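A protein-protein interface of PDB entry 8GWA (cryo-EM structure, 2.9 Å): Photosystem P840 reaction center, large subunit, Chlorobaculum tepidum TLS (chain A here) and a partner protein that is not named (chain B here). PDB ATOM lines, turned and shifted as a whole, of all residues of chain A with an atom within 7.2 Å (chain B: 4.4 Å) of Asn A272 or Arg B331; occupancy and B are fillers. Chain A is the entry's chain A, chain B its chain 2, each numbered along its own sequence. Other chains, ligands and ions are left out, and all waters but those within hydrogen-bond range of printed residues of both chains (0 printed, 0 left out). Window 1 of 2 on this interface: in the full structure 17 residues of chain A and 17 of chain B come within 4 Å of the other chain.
The guanidinium group of Arg B331 lies within hydrogen-bond range of the backbone carbonyl oxygen of Asn A272 (2.6 Å).
The guanidinium group (NH1) of Arg B331 is in salt-bridge range of the side-chain carboxylate (OD2) of Asp A274, 3.0 Å away.
The backbone NH (N) of Gln B333 lies within hydrogen-bond range of the backbone carbonyl oxygen (O) of Glu A68 (3.2 Å).
The side-chain amide oxygen of Gln B329 lies close to the side-chain carboxylate of Asp A273 (3.2 Å).
NH1 of Arg B331 lies within salt-bridge range of OD2 of Asp A72, at 3.2 Å.
The guanidinium group of Arg B331 sits at hydrogen-bond distance from the backbone carbonyl oxygen of Leu A271, at 2.9 Å.
N of Ala B344 lies close to OD1 of Asn A272, 2.4 Å away.
OE1 of Gln B329 lies within hydrogen-bond range of NZ of Lys A397 (2.7 Å).
The side-chain carboxylate (OD1) of Asp A72 sits at hydrogen-bond distance from the side-chain hydroxyl (OH) of Tyr A202 (2.4 Å).
N of Arg B331 is in hydrogen-bond range of O of Arg B339.
N of Arg B339 is in hydrogen-bond range of O of Ser B332, at 3.4 Å.
Ser B332 touches Glu A68.
Gln B333 touches Lys A69 (O to CA, 3.3 Å).
Ser B332 touches Leu A70.
Leu A271 touches Gly B343.
Asn A272 touches Gly B342 (OD1 to O, 3.7 Å).
C of Gly B343 touches OD1 of Asn A272, at 3.3 Å.
Asn A272 touches Tyr B345 (OD1 to N, 3.9 Å).
Gln B329 touches Tyr A394.
Met A403 touches Gln B329.
Of chain B, only Arg B331 (2.6 Å), Gly B342 (3.7 Å), Gly B343 (3.3 Å), Ala B344 (2.4 Å) and Tyr B345 (3.9 Å) come within 4 Å of Asn A272.
Of the printed residues of chain B, Lys A397 touches Gln B329 (2.7 Å).
Ile A407 touches none of the printed residues of chain B.
Of chain A, only Asp A72, Leu A271, Asn A272 and Asp A274 come within 4 Å of Arg B331.
Printed residues of chain A within 4 Å of Ser B332: Glu A68 and Leu A70.
Of the printed residues of chain A, Gln B333 touches Glu A68 and Lys A69.
The nearest residue of chain A that does not touch Arg B331 is Asp A273 (4.03 Å).
The nearest printed residue of chain B that does not touch Asp A273 is Arg B331 (4.03 Å).
Among the printed residues, 17 pairs touch across the chains.
Among the printed residues, Asp or Glu carboxylates within 4 Å of a Lys or Arg side-chain nitrogen of the other chain: Asp A72 with Arg B331 and Asp A274 with Arg B331.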
ATOM      1  N   THR A  67     -26.680 -19.027 -14.342  1.00  0.00           N
ATOM      2  CA  THR A  67     -26.126 -19.027 -12.994  1.00  0.00           C
ATOM      3  C   THR A  67     -24.628 -19.303 -12.960  1.00  0.00           C
ATOM      4  O   THR A  67     -24.004 -19.070 -11.920  1.00  0.00           O
ATOM      5  CB  THR A  67     -26.860 -20.049 -12.133  1.00  0.00           C
ATOM      6  OG1 THR A  67     -26.740 -21.351 -12.722  1.00  0.00           O
ATOM      7  CG2 THR A  67     -28.325 -19.687 -12.001  1.00  0.00           C
ATOM      8  N   GLU A  68     -24.038 -19.785 -14.056  1.00  0.00           N
ATOM      9  CA  GLU A  68     -22.598 -20.020 -14.073  1.00  0.00           C
ATOM     10  C   GLU A  68     -21.825 -18.721 -13.878  1.00  0.00           C
ATOM     11  O   GLU A  68     -20.826 -18.689 -13.150  1.00  0.00           O
ATOM     12  CB  GLU A  68     -22.189 -20.697 -15.381  1.00  0.00           C
ATOM     13  CG  GLU A  68     -22.735 -22.104 -15.550  1.00  0.00           C
ATOM     14  CD  GLU A  68     -22.152 -23.079 -14.546  1.00  0.00           C
ATOM     15  OE1 GLU A  68     -20.981 -22.897 -14.149  1.00  0.00           O
ATOM     16  OE2 GLU A  68     -22.864 -24.028 -14.155  1.00  0.00           O
ATOM     17  N   LYS A  69     -22.271 -17.643 -14.516  1.00  0.00           N
ATOM     18  CA  LYS A  69     -21.618 -16.346 -14.409  1.00  0.00           C
ATOM     19  C   LYS A  69     -22.170 -15.498 -13.269  1.00  0.00           C
ATOM     20  O   LYS A  69     -21.776 -14.335 -13.131  1.00  0.00           O
ATOM     21  CB  LYS A  69     -21.739 -15.584 -15.730  1.00  0.00           C
ATOM     22  CG  LYS A  69     -23.165 -15.414 -16.218  1.00  0.00           C
ATOM     23  CD  LYS A  69     -23.218 -15.233 -17.723  1.00  0.00           C
ATOM     24  CE  LYS A  69     -22.971 -16.546 -18.443  1.00  0.00           C
ATOM     25  NZ  LYS A  69     -23.113 -16.404 -19.917  1.00  0.00           N
ATOM     26  N   LEU A  70     -23.067 -16.046 -12.456  1.00  0.00           N
ATOM     27  CA  LEU A  70     -23.648 -15.336 -11.326  1.00  0.00           C
ATOM     28  C   LEU A  70     -23.090 -15.892 -10.024  1.00  0.00           C
ATOM     29  O   LEU A  70     -22.846 -17.097  -9.906  1.00  0.00           O
ATOM     30  CB  LEU A  70     -25.174 -15.453 -11.321  1.00  0.00           C
ATOM     31  CG  LEU A  70     -25.926 -14.869 -12.518  1.00  0.00           C
ATOM     32  CD1 LEU A  70     -27.426 -14.934 -12.285  1.00  0.00           C
ATOM     33  CD2 LEU A  70     -25.485 -13.439 -12.786  1.00  0.00           C
ATOM     34  N   ASP A  71     -22.880 -15.009  -9.054  1.00  0.00           N
ATOM     35  CA  ASP A  71     -22.486 -15.406  -7.715  1.00  0.00           C
ATOM     36  C   ASP A  71     -23.707 -15.391  -6.797  1.00  0.00           C
ATOM     37  O   ASP A  71     -24.836 -15.137  -7.225  1.00  0.00           O
ATOM     38  CB  ASP A  71     -21.371 -14.497  -7.193  1.00  0.00           C
ATOM     39  CG  ASP A  71     -21.743 -13.029  -7.238  1.00  0.00           C
ATOM     40  OD1 ASP A  71     -22.680 -12.623  -6.521  1.00  0.00           O
ATOM     41  OD2 ASP A  71     -21.092 -12.275  -7.991  1.00  0.00           O
ATOM     42  N   ASP A  72     -23.472 -15.669  -5.514  1.00  0.00           N
ATOM     43  CA  ASP A  72     -24.568 -15.727  -4.551  1.00  0.00           C
ATOM     44  C   ASP A  72     -25.234 -14.365  -4.389  1.00  0.00           C
ATOM     45  O   ASP A  72     -26.465 -14.251  -4.439  1.00  0.00           O
ATOM     46  CB  ASP A  72     -24.047 -16.230  -3.204  1.00  0.00           C
ATOM     47  CG  ASP A  72     -23.151 -17.444  -3.340  1.00  0.00           C
ATOM     48  OD1 ASP A  72     -23.474 -18.334  -4.154  1.00  0.00           O
ATOM     49  OD2 ASP A  72     -22.126 -17.506  -2.630  1.00  0.00           O
ATOM     50  N   LYS A 200     -21.986 -18.889   5.659  1.00  0.00           N
ATOM     51  CA  LYS A 200     -20.951 -18.930   4.639  1.00  0.00           C
ATOM     52  C   LYS A 200     -21.264 -19.910   3.521  1.00  0.00           C
ATOM     53  O   LYS A 200     -20.665 -19.814   2.445  1.00  0.00           O
ATOM     54  CB  LYS A 200     -19.603 -19.306   5.267  1.00  0.00           C
ATOM     55  CG  LYS A 200     -19.264 -18.527   6.526  1.00  0.00           C
ATOM     56  CD  LYS A 200     -19.262 -17.032   6.277  1.00  0.00           C
ATOM     57  CE  LYS A 200     -18.594 -16.289   7.420  1.00  0.00           C
ATOM     58  NZ  LYS A 200     -19.483 -15.251   8.006  1.00  0.00           N
ATOM     59  N   SER A 201     -22.181 -20.843   3.755  1.00  0.00           N
ATOM     60  CA  SER A 201     -22.532 -21.870   2.790  1.00  0.00           C
ATOM     61  C   SER A 201     -24.048 -22.005   2.729  1.00  0.00           C
ATOM     62  O   SER A 201     -24.764 -21.615   3.654  1.00  0.00           O
ATOM     63  CB  SER A 201     -21.882 -23.212   3.150  1.00  0.00           C
ATOM     64  OG  SER A 201     -22.474 -23.773   4.307  1.00  0.00           O
ATOM     65  N   TYR A 202     -24.531 -22.561   1.616  1.00  0.00           N
ATOM     66  CA  TYR A 202     -25.971 -22.621   1.380  1.00  0.00           C
ATOM     67  C   TYR A 202     -26.675 -23.527   2.384  1.00  0.00           C
ATOM     68  O   TYR A 202     -27.763 -23.192   2.867  1.00  0.00           O
ATOM     69  CB  TYR A 202     -26.247 -23.071  -0.052  1.00  0.00           C
ATOM     70  CG  TYR A 202     -26.129 -21.953  -1.063  1.00  0.00           C
ATOM     71  CD1 TYR A 202     -25.104 -21.021  -0.984  1.00  0.00           C
ATOM     72  CD2 TYR A 202     -27.053 -21.818  -2.086  1.00  0.00           C
ATOM     73  CE1 TYR A 202     -24.999 -19.995  -1.899  1.00  0.00           C
ATOM     74  CE2 TYR A 202     -26.955 -20.794  -3.007  1.00  0.00           C
ATOM     75  CZ  TYR A 202     -25.926 -19.888  -2.909  1.00  0.00           C
ATOM     76  OH  TYR A 202     -25.826 -18.867  -3.824  1.00  0.00           O
ATOM     77  N   ALA A 268     -24.615 -31.875   0.788  1.00  0.00           N
ATOM     78  CA  ALA A 268     -23.205 -31.939   0.420  1.00  0.00           C
ATOM     79  C   ALA A 268     -22.922 -31.310  -0.937  1.00  0.00           C
ATOM     80  O   ALA A 268     -22.264 -30.268  -1.022  1.00  0.00           O
ATOM     81  CB  ALA A 268     -22.715 -33.389   0.438  1.00  0.00           C
ATOM     82  N   ILE A 269     -23.415 -31.941  -1.999  1.00  0.00           N
ATOM     83  CA  ILE A 269     -23.020 -31.557  -3.349  1.00  0.00           C
ATOM     84  C   ILE A 269     -23.640 -30.235  -3.777  1.00  0.00           C
ATOM     85  O   ILE A 269     -23.041 -29.497  -4.568  1.00  0.00           O
ATOM     86  CB  ILE A 269     -23.374 -32.695  -4.314  1.00  0.00           C
ATOM     87  CG1 ILE A 269     -24.856 -32.639  -4.670  1.00  0.00           C
ATOM     88  CG2 ILE A 269     -23.042 -34.010  -3.667  1.00  0.00           C
ATOM     89  CD1 ILE A 269     -25.270 -33.662  -5.652  1.00  0.00           C
ATOM     90  N   HIS A 270     -24.834 -29.906  -3.279  1.00  0.00           N
ATOM     91  CA  HIS A 270     -25.467 -28.648  -3.648  1.00  0.00           C
ATOM     92  C   HIS A 270     -24.714 -27.447  -3.109  1.00  0.00           C
ATOM     93  O   HIS A 270     -25.001 -26.320  -3.520  1.00  0.00           O
ATOM     94  CB  HIS A 270     -26.910 -28.619  -3.154  1.00  0.00           C
ATOM     95  CG  HIS A 270     -27.737 -29.749  -3.671  1.00  0.00           C
ATOM     96  ND1 HIS A 270     -27.553 -30.284  -4.927  1.00  0.00           N
ATOM     97  CD2 HIS A 270     -28.751 -30.447  -3.109  1.00  0.00           C
ATOM     98  CE1 HIS A 270     -28.411 -31.268  -5.113  1.00  0.00           C
ATOM     99  NE2 HIS A 270     -29.153 -31.386  -4.025  1.00  0.00           N
ATOM    100  N   LEU A 271     -23.776 -27.662  -2.193  1.00  0.00           N
ATOM    101  CA  LEU A 271     -23.016 -26.557  -1.633  1.00  0.00           C
ATOM    102  C   LEU A 271     -22.054 -25.963  -2.654  1.00  0.00           C
ATOM    103  O   LEU A 271     -21.805 -24.752  -2.639  1.00  0.00           O
ATOM    104  CB  LEU A 271     -22.252 -27.033  -0.402  1.00  0.00           C
ATOM    105  CG  LEU A 271     -23.013 -27.085   0.921  1.00  0.00           C
ATOM    106  CD1 LEU A 271     -23.421 -25.689   1.291  1.00  0.00           C
ATOM    107  CD2 LEU A 271     -24.221 -28.011   0.874  1.00  0.00           C
ATOM    108  N   ASN A 272     -21.512 -26.792  -3.547  1.00  0.00           N
ATOM    109  CA  ASN A 272     -20.459 -26.330  -4.444  1.00  0.00           C
ATOM    110  C   ASN A 272     -21.033 -25.577  -5.636  1.00  0.00           C
ATOM    111  O   ASN A 272     -20.783 -24.380  -5.805  1.00  0.00           O
ATOM    112  CB  ASN A 272     -19.627 -27.521  -4.923  1.00  0.00           C
ATOM    113  CG  ASN A 272     -18.786 -28.119  -3.823  1.00  0.00           C
ATOM    114  OD1 ASN A 272     -18.189 -27.400  -3.023  1.00  0.00           O
ATOM    115  ND2 ASN A 272     -18.738 -29.445  -3.771  1.00  0.00           N
ATOM    116  N   ASP A 273     -21.801 -26.263  -6.475  1.00  0.00           N
ATOM    117  CA  ASP A 273     -22.464 -25.626  -7.611  1.00  0.00           C
ATOM    118  C   ASP A 273     -23.929 -25.347  -7.288  1.00  0.00           C
ATOM    119  O   ASP A 273     -24.848 -25.799  -7.970  1.00  0.00           O
ATOM    120  CB  ASP A 273     -22.326 -26.491  -8.860  1.00  0.00           C
ATOM    121  CG  ASP A 273     -22.378 -25.680 -10.138  1.00  0.00           C
ATOM    122  OD1 ASP A 273     -22.479 -24.438 -10.052  1.00  0.00           O
ATOM    123  OD2 ASP A 273     -22.330 -26.285 -11.228  1.00  0.00           O
ATOM    124  N   ASP A 274     -24.134 -24.579  -6.218  1.00  0.00           N
ATOM    125  CA  ASP A 274     -25.482 -24.178  -5.837  1.00  0.00           C
ATOM    126  C   ASP A 274     -26.157 -23.346  -6.916  1.00  0.00           C
ATOM    127  O   ASP A 274     -27.389 -23.246  -6.932  1.00  0.00           O
ATOM    128  CB  ASP A 274     -25.435 -23.410  -4.520  1.00  0.00           C
ATOM    129  CG  ASP A 274     -24.319 -22.384  -4.479  1.00  0.00           C
ATOM    130  OD1 ASP A 274     -24.154 -21.635  -5.463  1.00  0.00           O
ATOM    131  OD2 ASP A 274     -23.599 -22.329  -3.461  1.00  0.00           O
ATOM    132  N   MET A 275     -25.372 -22.739  -7.805  1.00  0.00           N
ATOM    133  CA  MET A 275     -25.929 -22.039  -8.954  1.00  0.00           C
ATOM    134  C   MET A 275     -26.811 -22.940  -9.809  1.00  0.00           C
ATOM    135  O   MET A 275     -27.810 -22.473 -10.367  1.00  0.00           O
ATOM    136  CB  MET A 275     -24.793 -21.446  -9.784  1.00  0.00           C
ATOM    137  CG  MET A 275     -24.006 -20.351  -9.081  1.00  0.00           C
ATOM    138  SD  MET A 275     -25.059 -18.934  -8.689  1.00  0.00           S
ATOM    139  CE  MET A 275     -25.369 -19.157  -6.944  1.00  0.00           C
ATOM    140  N   LYS A 276     -26.477 -24.223  -9.925  1.00  0.00           N
ATOM    141  CA  LYS A 276     -27.269 -25.091 -10.787  1.00  0.00           C
ATOM    142  C   LYS A 276     -27.775 -26.328 -10.057  1.00  0.00           C
ATOM    143  O   LYS A 276     -28.874 -26.809 -10.346  1.00  0.00           O
ATOM    144  CB  LYS A 276     -26.460 -25.497 -12.019  1.00  0.00           C
ATOM    145  CG  LYS A 276     -27.323 -25.911 -13.199  1.00  0.00           C
ATOM    146  CD  LYS A 276     -27.862 -24.702 -13.940  1.00  0.00           C
ATOM    147  CE  LYS A 276     -26.801 -24.089 -14.834  1.00  0.00           C
ATOM    148  NZ  LYS A 276     -27.274 -22.823 -15.451  1.00  0.00           N
ATOM    149  N   ALA A 277     -26.993 -26.857  -9.118  1.00  0.00           N
ATOM    150  CA  ALA A 277     -27.428 -28.045  -8.388  1.00  0.00           C
ATOM    151  C   ALA A 277     -28.531 -27.705  -7.394  1.00  0.00           C
ATOM    152  O   ALA A 277     -29.659 -28.207  -7.496  1.00  0.00           O
ATOM    153  CB  ALA A 277     -26.237 -28.691  -7.676  1.00  0.00           C
ATOM    154  N   TYR A 394     -26.238 -29.314 -14.830  1.00  0.00           N
ATOM    155  CA  TYR A 394     -25.163 -29.412 -13.846  1.00  0.00           C
ATOM    156  C   TYR A 394     -24.559 -30.809 -13.822  1.00  0.00           C
ATOM    157  O   TYR A 394     -23.343 -30.973 -13.656  1.00  0.00           O
ATOM    158  CB  TYR A 394     -25.688 -29.032 -12.462  1.00  0.00           C
ATOM    159  CG  TYR A 394     -24.930 -29.664 -11.315  1.00  0.00           C
ATOM    160  CD1 TYR A 394     -23.779 -29.080 -10.809  1.00  0.00           C
ATOM    161  CD2 TYR A 394     -25.380 -30.837 -10.724  1.00  0.00           C
ATOM    162  CE1 TYR A 394     -23.091 -29.658  -9.760  1.00  0.00           C
ATOM    163  CE2 TYR A 394     -24.699 -31.419  -9.675  1.00  0.00           C
ATOM    164  CZ  TYR A 394     -23.555 -30.823  -9.196  1.00  0.00           C
ATOM    165  OH  TYR A 394     -22.873 -31.399  -8.150  1.00  0.00           O
ATOM    166  N   LYS A 397     -22.341 -31.347 -16.651  1.00  0.00           N
ATOM    167  CA  LYS A 397     -21.127 -30.577 -16.408  1.00  0.00           C
ATOM    168  C   LYS A 397     -20.180 -31.310 -15.466  1.00  0.00           C
ATOM    169  O   LYS A 397     -18.959 -31.246 -15.643  1.00  0.00           O
ATOM    170  CB  LYS A 397     -21.467 -29.198 -15.846  1.00  0.00           C
ATOM    171  CG  LYS A 397     -20.324 -28.201 -15.967  1.00  0.00           C
ATOM    172  CD  LYS A 397     -20.665 -26.873 -15.321  1.00  0.00           C
ATOM    173  CE  LYS A 397     -20.473 -26.931 -13.816  1.00  0.00           C
ATOM    174  NZ  LYS A 397     -19.044 -27.117 -13.440  1.00  0.00           N
ATOM    175  N   MET A 403     -16.248 -35.046 -12.066  1.00  0.00           N
ATOM    176  CA  MET A 403     -16.797 -34.830 -10.733  1.00  0.00           C
ATOM    177  C   MET A 403     -17.983 -35.747 -10.453  1.00  0.00           C
ATOM    178  O   MET A 403     -18.370 -35.905  -9.291  1.00  0.00           O
ATOM    179  CB  MET A 403     -17.202 -33.362 -10.577  1.00  0.00           C
ATOM    180  CG  MET A 403     -17.605 -32.937  -9.173  1.00  0.00           C
ATOM    181  SD  MET A 403     -16.282 -33.158  -7.971  1.00  0.00           S
ATOM    182  CE  MET A 403     -15.165 -31.846  -8.460  1.00  0.00           C
ATOM    183  N   ILE A 407     -18.886 -37.574  -6.501  1.00  0.00           N
ATOM    184  CA  ILE A 407     -20.009 -37.219  -5.645  1.00  0.00           C
ATOM    185  C   ILE A 407     -20.189 -38.292  -4.581  1.00  0.00           C
ATOM    186  O   ILE A 407     -20.183 -39.490  -4.885  1.00  0.00           O
ATOM    187  CB  ILE A 407     -21.291 -37.047  -6.472  1.00  0.00           C
ATOM    188  CG1 ILE A 407     -21.105 -35.951  -7.524  1.00  0.00           C
ATOM    189  CG2 ILE A 407     -22.469 -36.787  -5.567  1.00  0.00           C
ATOM    190  CD1 ILE A 407     -20.803 -34.592  -6.934  1.00  0.00           C
ATOM    191  N   GLN B 329     -14.785 -28.272  -6.945  1.00  0.00           N
ATOM    192  CA  GLN B 329     -15.366 -27.556  -8.072  1.00  0.00           C
ATOM    193  C   GLN B 329     -15.439 -26.059  -7.798  1.00  0.00           C
ATOM    194  O   GLN B 329     -15.764 -25.628  -6.689  1.00  0.00           O
ATOM    195  CB  GLN B 329     -16.762 -28.102  -8.370  1.00  0.00           C
ATOM    196  CG  GLN B 329     -17.417 -27.525  -9.610  1.00  0.00           C
ATOM    197  CD  GLN B 329     -18.835 -28.029  -9.799  1.00  0.00           C
ATOM    198  OE1 GLN B 329     -19.482 -27.735 -10.804  1.00  0.00           O
ATOM    199  NE2 GLN B 329     -19.325 -28.795  -8.831  1.00  0.00           N
ATOM    200  N   TYR B 330     -15.133 -25.267  -8.822  1.00  0.00           N
ATOM    201  CA  TYR B 330     -15.233 -23.820  -8.719  1.00  0.00           C
ATOM    202  C   TYR B 330     -16.695 -23.377  -8.693  1.00  0.00           C
ATOM    203  O   TYR B 330     -17.584 -24.029  -9.247  1.00  0.00           O
ATOM    204  CB  TYR B 330     -14.483 -23.151  -9.874  1.00  0.00           C
ATOM    205  CG  TYR B 330     -15.040 -23.456 -11.246  1.00  0.00           C
ATOM    206  CD1 TYR B 330     -14.587 -24.551 -11.969  1.00  0.00           C
ATOM    207  CD2 TYR B 330     -16.004 -22.644 -11.826  1.00  0.00           C
ATOM    208  CE1 TYR B 330     -15.086 -24.837 -13.223  1.00  0.00           C
ATOM    209  CE2 TYR B 330     -16.510 -22.922 -13.083  1.00  0.00           C
ATOM    210  CZ  TYR B 330     -16.047 -24.020 -13.776  1.00  0.00           C
ATOM    211  OH  TYR B 330     -16.545 -24.303 -15.027  1.00  0.00           O
ATOM    212  N   ARG B 331     -16.933 -22.241  -8.034  1.00  0.00           N
ATOM    213  CA  ARG B 331     -18.292 -21.732  -7.869  1.00  0.00           C
ATOM    214  C   ARG B 331     -18.799 -21.030  -9.122  1.00  0.00           C
ATOM    215  O   ARG B 331     -19.766 -21.478  -9.748  1.00  0.00           O
ATOM    216  CB  ARG B 331     -18.356 -20.788  -6.664  1.00  0.00           C
ATOM    217  CG  ARG B 331     -19.746 -20.231  -6.384  1.00  0.00           C
ATOM    218  CD  ARG B 331     -20.738 -21.303  -5.980  1.00  0.00           C
ATOM    219  NE  ARG B 331     -20.346 -22.020  -4.773  1.00  0.00           N
ATOM    220  CZ  ARG B 331     -20.594 -21.598  -3.542  1.00  0.00           C
ATOM    221  NH1 ARG B 331     -21.219 -20.455  -3.315  1.00  0.00           N
ATOM    222  NH2 ARG B 331     -20.208 -22.344  -2.510  1.00  0.00           N
ATOM    223  N   SER B 332     -18.165 -19.925  -9.506  1.00  0.00           N
ATOM    224  CA  SER B 332     -18.690 -19.081 -10.572  1.00  0.00           C
ATOM    225  C   SER B 332     -17.574 -18.703 -11.529  1.00  0.00           C
ATOM    226  O   SER B 332     -16.644 -17.985 -11.150  1.00  0.00           O
ATOM    227  CB  SER B 332     -19.352 -17.824  -9.999  1.00  0.00           C
ATOM    228  OG  SER B 332     -18.380 -16.893  -9.560  1.00  0.00           O
ATOM    229  N   GLN B 333     -17.670 -19.187 -12.764  1.00  0.00           N
ATOM    230  CA  GLN B 333     -16.783 -18.747 -13.832  1.00  0.00           C
ATOM    231  C   GLN B 333     -17.262 -17.398 -14.350  1.00  0.00           C
ATOM    232  O   GLN B 333     -18.447 -17.232 -14.659  1.00  0.00           O
ATOM    233  CB  GLN B 333     -16.752 -19.780 -14.956  1.00  0.00           C
ATOM    234  CG  GLN B 333     -15.741 -19.482 -16.048  1.00  0.00           C
ATOM    235  CD  GLN B 333     -16.388 -19.004 -17.330  1.00  0.00           C
ATOM    236  OE1 GLN B 333     -17.449 -19.489 -17.720  1.00  0.00           O
ATOM    237  NE2 GLN B 333     -15.748 -18.049 -17.995  1.00  0.00           N
ATOM    238  N   ARG B 339     -13.810 -18.580  -9.380  1.00  0.00           N
ATOM    239  CA  ARG B 339     -14.012 -18.372  -7.953  1.00  0.00           C
ATOM    240  C   ARG B 339     -14.289 -19.693  -7.250  1.00  0.00           C
ATOM    241  O   ARG B 339     -15.058 -20.524  -7.743  1.00  0.00           O
ATOM    242  CB  ARG B 339     -15.169 -17.403  -7.688  1.00  0.00           C
ATOM    243  CG  ARG B 339     -14.904 -15.962  -8.085  1.00  0.00           C
ATOM    244  CD  ARG B 339     -16.196 -15.151  -8.034  1.00  0.00           C
ATOM    245  NE  ARG B 339     -16.032 -13.758  -8.436  1.00  0.00           N
ATOM    246  CZ  ARG B 339     -15.232 -12.880  -7.842  1.00  0.00           C
ATOM    247  NH1 ARG B 339     -14.541 -13.193  -6.758  1.00  0.00           N
ATOM    248  NH2 ARG B 339     -15.142 -11.648  -8.336  1.00  0.00           N
ATOM    249  N   TRP B 340     -13.656 -19.874  -6.094  1.00  0.00           N
ATOM    250  CA  TRP B 340     -13.929 -20.984  -5.191  1.00  0.00           C
ATOM    251  C   TRP B 340     -14.401 -20.408  -3.866  1.00  0.00           C
ATOM    252  O   TRP B 340     -13.762 -19.503  -3.322  1.00  0.00           O
ATOM    253  CB  TRP B 340     -12.685 -21.845  -4.966  1.00  0.00           C
ATOM    254  CG  TRP B 340     -12.354 -22.769  -6.090  1.00  0.00           C
ATOM    255  CD1 TRP B 340     -12.593 -24.109  -6.148  1.00  0.00           C
ATOM    256  CD2 TRP B 340     -11.703 -22.423  -7.315  1.00  0.00           C
ATOM    257  NE1 TRP B 340     -12.137 -24.618  -7.339  1.00  0.00           N
ATOM    258  CE2 TRP B 340     -11.586 -23.602  -8.073  1.00  0.00           C
ATOM    259  CE3 TRP B 340     -11.213 -21.229  -7.846  1.00  0.00           C
ATOM    260  CZ2 TRP B 340     -10.999 -23.621  -9.334  1.00  0.00           C
ATOM    261  CZ3 TRP B 340     -10.631 -21.250  -9.095  1.00  0.00           C
ATOM    262  CH2 TRP B 340     -10.529 -22.437  -9.826  1.00  0.00           C
ATOM    263  N   SER B 341     -15.510 -20.929  -3.348  1.00  0.00           N
ATOM    264  CA  SER B 341     -16.041 -20.450  -2.077  1.00  0.00           C
ATOM    265  C   SER B 341     -17.042 -21.440  -1.499  1.00  0.00           C
ATOM    266  O   SER B 341     -17.939 -21.904  -2.207  1.00  0.00           O
ATOM    267  CB  SER B 341     -16.696 -19.078  -2.250  1.00  0.00           C
ATOM    268  OG  SER B 341     -17.348 -18.670  -1.061  1.00  0.00           O
ATOM    269  N   GLY B 342     -16.891 -21.773  -0.222  1.00  0.00           N
ATOM    270  CA  GLY B 342     -17.838 -22.637   0.456  1.00  0.00           C
ATOM    271  C   GLY B 342     -17.883 -24.044  -0.116  1.00  0.00           C
ATOM    272  O   GLY B 342     -17.195 -24.396  -1.073  1.00  0.00           O
ATOM    273  N   GLY B 343     -18.723 -24.863   0.507  1.00  0.00           N
ATOM    274  CA  GLY B 343     -18.928 -26.217   0.018  1.00  0.00           C
ATOM    275  C   GLY B 343     -17.697 -27.076   0.206  1.00  0.00           C
ATOM    276  O   GLY B 343     -17.141 -27.174   1.306  1.00  0.00           O
ATOM    277  N   ALA B 344     -17.263 -27.718  -0.880  1.00  0.00           N
ATOM    278  CA  ALA B 344     -16.067 -28.548  -0.817  1.00  0.00           C
ATOM    279  C   ALA B 344     -14.799 -27.713  -0.732  1.00  0.00           C
ATOM    280  O   ALA B 344     -13.791 -28.188  -0.205  1.00  0.00           O
ATOM    281  CB  ALA B 344     -15.995 -29.480  -2.026  1.00  0.00           C
ATOM    282  N   TYR B 345     -14.818 -26.481  -1.246  1.00  0.00           N
ATOM    283  CA  TYR B 345     -13.629 -25.644  -1.138  1.00  0.00           C
ATOM    284  C   TYR B 345     -13.394 -25.199   0.298  1.00  0.00           C
ATOM    285  O   TYR B 345     -12.251 -25.181   0.764  1.00  0.00           O
ATOM    286  CB  TYR B 345     -13.726 -24.430  -2.056  1.00  0.00           C
ATOM    287  CG  TYR B 345     -12.496 -23.559  -1.966  1.00  0.00           C
ATOM    288  CD1 TYR B 345     -11.296 -23.967  -2.529  1.00  0.00           C
ATOM    289  CD2 TYR B 345     -12.527 -22.341  -1.304  1.00  0.00           C
ATOM    290  CE1 TYR B 345     -10.166 -23.185  -2.444  1.00  0.00           C
ATOM    291  CE2 TYR B 345     -11.398 -21.550  -1.215  1.00  0.00           C
ATOM    292  CZ  TYR B 345     -10.221 -21.977  -1.788  1.00  0.00           C
ATOM    293  OH  TYR B 345      -9.092 -21.199  -1.704  1.00  0.00           O
